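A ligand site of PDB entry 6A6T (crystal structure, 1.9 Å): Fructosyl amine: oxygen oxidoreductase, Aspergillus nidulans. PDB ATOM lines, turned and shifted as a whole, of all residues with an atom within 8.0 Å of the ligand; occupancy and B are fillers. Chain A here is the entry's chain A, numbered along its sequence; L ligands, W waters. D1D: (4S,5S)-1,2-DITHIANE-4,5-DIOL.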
ATOM      1  N   THR A 314       9.914  -9.429  -3.690  1.00  0.00           N
ATOM      2  CA  THR A 314       9.399 -10.704  -3.191  1.00  0.00           C
ATOM      3  C   THR A 314       8.136 -11.169  -3.915  1.00  0.00           C
ATOM      4  O   THR A 314       7.605 -12.238  -3.627  1.00  0.00           O
ATOM      5  CB  THR A 314       9.076 -10.637  -1.701  1.00  0.00           C
ATOM      6  OG1 THR A 314       8.128  -9.588  -1.477  1.00  0.00           O
ATOM      7  CG2 THR A 314      10.339 -10.355  -0.902  1.00  0.00           C
ATOM      8  N   ASP A 315       7.649 -10.351  -4.849  1.00  0.00           N
ATOM      9  CA  ASP A 315       6.564 -10.748  -5.722  1.00  0.00           C
ATOM     10  C   ASP A 315       7.091 -11.689  -6.805  1.00  0.00           C
ATOM     11  O   ASP A 315       8.239 -11.543  -7.241  1.00  0.00           O
ATOM     12  CB  ASP A 315       5.904  -9.537  -6.377  1.00  0.00           C
ATOM     13  CG  ASP A 315       4.867  -8.874  -5.497  1.00  0.00           C
ATOM     14  OD1 ASP A 315       4.924  -9.041  -4.253  1.00  0.00           O
ATOM     15  OD2 ASP A 315       3.994  -8.175  -6.039  1.00  0.00           O
ATOM     16  N   THR A 316       6.272 -12.638  -7.223  1.00  0.00           N
ATOM     17  CA  THR A 316       6.608 -13.484  -8.361  1.00  0.00           C
ATOM     18  C   THR A 316       5.552 -13.359  -9.453  1.00  0.00           C
ATOM     19  O   THR A 316       5.393 -12.302 -10.074  1.00  0.00           O
ATOM     20  CB  THR A 316       6.758 -14.962  -7.958  1.00  0.00           C
ATOM     21  OG1 THR A 316       5.608 -15.373  -7.214  1.00  0.00           O
ATOM     22  CG2 THR A 316       8.008 -15.150  -7.102  1.00  0.00           C
ATOM     23  N   TYR A 317       4.827 -14.450  -9.694  1.00  0.00           N
ATOM     24  CA  TYR A 317       3.722 -14.463 -10.630  1.00  0.00           C
ATOM     25  C   TYR A 317       2.613 -15.390 -10.099  1.00  0.00           C
ATOM     26  O   TYR A 317       2.838 -16.136  -9.148  1.00  0.00           O
ATOM     27  CB  TYR A 317       4.175 -14.908 -12.046  1.00  0.00           C
ATOM     28  CG  TYR A 317       5.071 -16.126 -12.164  1.00  0.00           C
ATOM     29  CD1 TYR A 317       4.702 -17.356 -11.627  1.00  0.00           C
ATOM     30  CD2 TYR A 317       6.234 -16.070 -12.920  1.00  0.00           C
ATOM     31  CE1 TYR A 317       5.505 -18.486 -11.771  1.00  0.00           C
ATOM     32  CE2 TYR A 317       7.026 -17.194 -13.080  1.00  0.00           C
ATOM     33  CZ  TYR A 317       6.674 -18.394 -12.506  1.00  0.00           C
ATOM     34  OH  TYR A 317       7.498 -19.488 -12.691  1.00  0.00           O
ATOM     35  N   PRO A 318       1.409 -15.322 -10.693  1.00  0.00           N
ATOM     36  CA  PRO A 318       0.339 -16.204 -10.214  1.00  0.00           C
ATOM     37  C   PRO A 318       0.656 -17.690 -10.411  1.00  0.00           C
ATOM     38  O   PRO A 318       1.549 -18.019 -11.201  1.00  0.00           O
ATOM     39  CB  PRO A 318      -0.856 -15.786 -11.076  1.00  0.00           C
ATOM     40  CG  PRO A 318      -0.569 -14.364 -11.452  1.00  0.00           C
ATOM     41  CD  PRO A 318       0.916 -14.321 -11.645  1.00  0.00           C
ATOM     42  N   HIS A 319      -0.063 -18.559  -9.709  1.00  0.00           N
ATOM     43  CA  HIS A 319       0.098 -20.001  -9.864  1.00  0.00           C
ATOM     44  C   HIS A 319      -0.217 -20.428 -11.293  1.00  0.00           C
ATOM     45  O   HIS A 319       0.441 -21.305 -11.835  1.00  0.00           O
ATOM     46  CB  HIS A 319      -0.801 -20.758  -8.877  1.00  0.00           C
ATOM     47  CG  HIS A 319      -0.382 -20.636  -7.444  1.00  0.00           C
ATOM     48  ND1 HIS A 319       0.925 -20.452  -7.057  1.00  0.00           N
ATOM     49  CD2 HIS A 319      -1.117 -20.647  -6.301  1.00  0.00           C
ATOM     50  CE1 HIS A 319       0.998 -20.367  -5.742  1.00  0.00           C
ATOM     51  NE2 HIS A 319      -0.230 -20.485  -5.262  1.00  0.00           N
ATOM     52  N   ALA A 320      -1.210 -19.783 -11.908  1.00  0.00           N
ATOM     53  CA  ALA A 320      -1.628 -20.142 -13.261  1.00  0.00           C
ATOM     54  C   ALA A 320      -0.499 -19.941 -14.265  1.00  0.00           C
ATOM     55  O   ALA A 320      -0.391 -20.691 -15.245  1.00  0.00           O
ATOM     56  CB  ALA A 320      -2.850 -19.339 -13.656  1.00  0.00           C
ATOM     57  N   SER A 321       0.338 -18.937 -14.023  1.00  0.00           N
ATOM     58  CA  SER A 321       1.468 -18.632 -14.884  1.00  0.00           C
ATOM     59  C   SER A 321       2.554 -19.687 -14.782  1.00  0.00           C
ATOM     60  O   SER A 321       3.216 -20.007 -15.772  1.00  0.00           O
ATOM     61  CB  SER A 321       2.048 -17.248 -14.552  1.00  0.00           C
ATOM     62  OG  SER A 321       1.105 -16.227 -14.828  1.00  0.00           O
ATOM     63  N   GLU A 322       2.760 -20.202 -13.573  1.00  0.00           N
ATOM     64  CA  GLU A 322       3.711 -21.283 -13.365  1.00  0.00           C
ATOM     65  C   GLU A 322       3.325 -22.449 -14.259  1.00  0.00           C
ATOM     66  O   GLU A 322       4.180 -23.038 -14.921  1.00  0.00           O
ATOM     67  CB  GLU A 322       3.732 -21.723 -11.895  1.00  0.00           C
ATOM     68  CG  GLU A 322       4.660 -22.884 -11.582  1.00  0.00           C
ATOM     69  CD  GLU A 322       6.092 -22.440 -11.309  1.00  0.00           C
ATOM     70  OE1 GLU A 322       6.881 -23.253 -10.786  1.00  0.00           O
ATOM     71  OE2 GLU A 322       6.433 -21.285 -11.617  1.00  0.00           O
ATOM     72  N   VAL A 323       2.033 -22.752 -14.310  1.00  0.00           N
ATOM     73  CA  VAL A 323       1.526 -23.859 -15.117  1.00  0.00           C
ATOM     74  C   VAL A 323       1.826 -23.651 -16.603  1.00  0.00           C
ATOM     75  O   VAL A 323       2.366 -24.529 -17.265  1.00  0.00           O
ATOM     76  CB  VAL A 323       0.009 -24.048 -14.941  1.00  0.00           C
ATOM     77  CG1 VAL A 323      -0.477 -25.272 -15.716  1.00  0.00           C
ATOM     78  CG2 VAL A 323      -0.347 -24.159 -13.467  1.00  0.00           C
ATOM     79  N   LYS A 326       5.540 -23.711 -17.557  1.00  0.00           N
ATOM     80  CA  LYS A 326       6.060 -25.083 -17.565  1.00  0.00           C
ATOM     81  C   LYS A 326       5.585 -25.852 -18.805  1.00  0.00           C
ATOM     82  O   LYS A 326       6.296 -26.730 -19.296  1.00  0.00           O
ATOM     83  CB  LYS A 326       5.673 -25.815 -16.276  1.00  0.00           C
ATOM     84  CG  LYS A 326       6.370 -25.251 -15.031  1.00  0.00           C
ATOM     85  CD  LYS A 326       6.036 -26.019 -13.771  1.00  0.00           C
ATOM     86  CE  LYS A 326       6.738 -27.375 -13.740  1.00  0.00           C
ATOM     87  NZ  LYS A 326       8.226 -27.221 -13.723  1.00  0.00           N
ATOM     88  N   GLU A 340      15.045 -26.087 -12.415  1.00  0.00           N
ATOM     89  CA  GLU A 340      14.308 -25.261 -11.465  1.00  0.00           C
ATOM     90  C   GLU A 340      14.083 -23.869 -12.027  1.00  0.00           C
ATOM     91  O   GLU A 340      15.004 -23.223 -12.522  1.00  0.00           O
ATOM     92  CB  GLU A 340      15.057 -25.177 -10.127  1.00  0.00           C
ATOM     93  CG  GLU A 340      14.178 -24.790  -8.947  1.00  0.00           C
ATOM     94  CD  GLU A 340      14.928 -24.861  -7.616  1.00  0.00           C
ATOM     95  OE1 GLU A 340      16.138 -24.553  -7.606  1.00  0.00           O
ATOM     96  OE2 GLU A 340      14.307 -25.216  -6.584  1.00  0.00           O
ATOM     97  N   LEU A 341      12.840 -23.411 -11.973  1.00  0.00           N
ATOM     98  CA  LEU A 341      12.529 -22.047 -12.415  1.00  0.00           C
ATOM     99  C   LEU A 341      12.945 -21.042 -11.343  1.00  0.00           C
ATOM    100  O   LEU A 341      12.828 -21.328 -10.156  1.00  0.00           O
ATOM    101  CB  LEU A 341      11.030 -21.916 -12.723  1.00  0.00           C
ATOM    102  CG  LEU A 341      10.504 -22.399 -14.079  1.00  0.00           C
ATOM    103  CD1 LEU A 341      10.746 -23.897 -14.290  1.00  0.00           C
ATOM    104  CD2 LEU A 341       9.021 -22.082 -14.197  1.00  0.00           C
ATOM    105  N   PHE A 342      13.438 -19.883 -11.765  1.00  0.00           N
ATOM    106  CA  PHE A 342      13.804 -18.841 -10.810  1.00  0.00           C
ATOM    107  C   PHE A 342      13.783 -17.461 -11.466  1.00  0.00           C
ATOM    108  O   PHE A 342      13.615 -17.348 -12.686  1.00  0.00           O
ATOM    109  CB  PHE A 342      15.180 -19.129 -10.194  1.00  0.00           C
ATOM    110  CG  PHE A 342      16.314 -19.019 -11.170  1.00  0.00           C
ATOM    111  CD1 PHE A 342      16.723 -20.114 -11.907  1.00  0.00           C
ATOM    112  CD2 PHE A 342      16.982 -17.806 -11.337  1.00  0.00           C
ATOM    113  CE1 PHE A 342      17.774 -20.006 -12.795  1.00  0.00           C
ATOM    114  CE2 PHE A 342      18.027 -17.695 -12.233  1.00  0.00           C
ATOM    115  CZ  PHE A 342      18.428 -18.790 -12.964  1.00  0.00           C
ATOM    116  N   ARG A 344      11.428 -15.588 -11.175  1.00  0.00           N
ATOM    117  CA  ARG A 344      10.019 -15.391 -11.486  1.00  0.00           C
ATOM    118  C   ARG A 344       9.635 -13.942 -11.291  1.00  0.00           C
ATOM    119  O   ARG A 344       9.851 -13.387 -10.209  1.00  0.00           O
ATOM    120  CB  ARG A 344       9.164 -16.283 -10.597  1.00  0.00           C
ATOM    121  CG  ARG A 344       9.476 -17.763 -10.671  1.00  0.00           C
ATOM    122  CD  ARG A 344       8.740 -18.478  -9.556  1.00  0.00           C
ATOM    123  NE  ARG A 344       8.677 -19.912  -9.774  1.00  0.00           N
ATOM    124  CZ  ARG A 344       9.499 -20.790  -9.221  1.00  0.00           C
ATOM    125  NH1 ARG A 344      10.455 -20.400  -8.384  1.00  0.00           N
ATOM    126  NH2 ARG A 344       9.353 -22.077  -9.504  1.00  0.00           N
ATOM    127  N   PRO A 430      -4.399 -16.187  -7.541  1.00  0.00           N
ATOM    128  CA  PRO A 430      -3.590 -16.371  -6.324  1.00  0.00           C
ATOM    129  C   PRO A 430      -2.168 -16.907  -6.583  1.00  0.00           C
ATOM    130  O   PRO A 430      -1.970 -17.686  -7.512  1.00  0.00           O
ATOM    131  CB  PRO A 430      -4.406 -17.388  -5.525  1.00  0.00           C
ATOM    132  CG  PRO A 430      -5.108 -18.194  -6.568  1.00  0.00           C
ATOM    133  CD  PRO A 430      -5.417 -17.237  -7.689  1.00  0.00           C
ATOM    134  N   GLY A 431      -1.205 -16.470  -5.773  1.00  0.00           N
ATOM    135  CA  GLY A 431       0.098 -17.096  -5.739  1.00  0.00           C
ATOM    136  C   GLY A 431       1.298 -16.188  -5.888  1.00  0.00           C
ATOM    137  O   GLY A 431       2.427 -16.616  -5.635  1.00  0.00           O
ATOM    138  N   TRP A 432       1.080 -14.937  -6.286  1.00  0.00           N
ATOM    139  CA  TRP A 432       2.204 -14.082  -6.646  1.00  0.00           C
ATOM    140  C   TRP A 432       2.777 -13.297  -5.474  1.00  0.00           C
ATOM    141  O   TRP A 432       3.816 -12.662  -5.604  1.00  0.00           O
ATOM    142  CB  TRP A 432       1.778 -13.114  -7.754  1.00  0.00           C
ATOM    143  CG  TRP A 432       0.461 -12.457  -7.529  1.00  0.00           C
ATOM    144  CD1 TRP A 432      -0.763 -12.993  -7.773  1.00  0.00           C
ATOM    145  CD2 TRP A 432       0.234 -11.137  -7.042  1.00  0.00           C
ATOM    146  NE1 TRP A 432      -1.751 -12.080  -7.464  1.00  0.00           N
ATOM    147  CE2 TRP A 432      -1.161 -10.934  -7.008  1.00  0.00           C
ATOM    148  CE3 TRP A 432       1.068 -10.096  -6.627  1.00  0.00           C
ATOM    149  CZ2 TRP A 432      -1.739  -9.737  -6.576  1.00  0.00           C
ATOM    150  CZ3 TRP A 432       0.501  -8.911  -6.196  1.00  0.00           C
ATOM    151  CH2 TRP A 432      -0.888  -8.751  -6.168  1.00  0.00           C
ATOM    152  N   ARG A 433       2.105 -13.353  -4.330  1.00  0.00           N
ATOM    153  CA  ARG A 433       2.538 -12.603  -3.157  1.00  0.00           C
ATOM    154  C   ARG A 433       3.119 -13.513  -2.080  1.00  0.00           C
ATOM    155  O   ARG A 433       4.310 -13.433  -1.773  1.00  0.00           O
ATOM    156  CB  ARG A 433       1.382 -11.784  -2.586  1.00  0.00           C
ATOM    157  CG  ARG A 433       0.229 -11.605  -3.544  1.00  0.00           C
ATOM    158  CD  ARG A 433      -0.703 -10.498  -3.075  1.00  0.00           C
ATOM    159  NE  ARG A 433      -2.042 -10.655  -3.651  1.00  0.00           N
ATOM    160  CZ  ARG A 433      -3.002 -11.423  -3.134  1.00  0.00           C
ATOM    161  NH1 ARG A 433      -2.788 -12.107  -2.020  1.00  0.00           N
ATOM    162  NH2 ARG A 433      -4.174 -11.503  -3.743  1.00  0.00           N
HETATM  163  S1  D1D L   1       4.125 -21.179  -8.148  1.00  0.00           S
HETATM  164  C1  D1D L   1       5.847 -21.487  -7.919  1.00  0.00           C
HETATM  165  C2  D1D L   1       6.374 -20.747  -6.689  1.00  0.00           C
HETATM  166  O2  D1D L   1       7.712 -21.173  -6.410  1.00  0.00           O
HETATM  167  C3  D1D L   1       6.373 -19.228  -6.902  1.00  0.00           C
HETATM  168  O3  D1D L   1       7.084 -18.619  -5.822  1.00  0.00           O
HETATM  169  C4  D1D L   1       4.958 -18.687  -6.961  1.00  0.00           C
HETATM  170  S4  D1D L   1       4.170 -19.199  -8.457  1.00  0.00           S
HETATM  171  O   HOH W   1       9.830 -18.082  -4.414  1.00  0.00           O
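The guanidinium group (NH1) of Arg 344 sits close to an oxygen (O2) of the ligand. ND1 of His 319 lies close to S1 of the ligand (3.5 Å).
The guanidinium group (NE) of Arg 344 sits at hydrogen-bond distance from the side-chain hydroxyl (OH) of Tyr 317 (3.2 Å). The side-chain carboxylate (OE1) of Glu 322 lies within salt-bridge range of the guanidinium group (NH2) of Arg 344 (3.0 Å). The guanidinium group (NH1) of Arg 344 is in hydrogen-bond range of the backbone carbonyl oxygen (O) of Leu 341 (3.1 Å). The backbone carbonyl oxygen of Trp 432 lies within hydrogen-bond range of the backbone NH of Thr 316 (2.9 Å). O of Pro 430 is in hydrogen-bond range of N of His 319, 3.0 Å away.
The backbone carbonyl oxygen (O) of Tyr 317 sits close to a sulfur (S4) of the ligand (3.4 Å). Residues that only touch the ligand: Thr 316, Pro 318, Glu 322 and Gly 431. Hydrophobic or aromatic side chains that line the ligand: Tyr 317. The nearest printed residue that does not touch the ligand is Trp 432 (5.4 Å).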
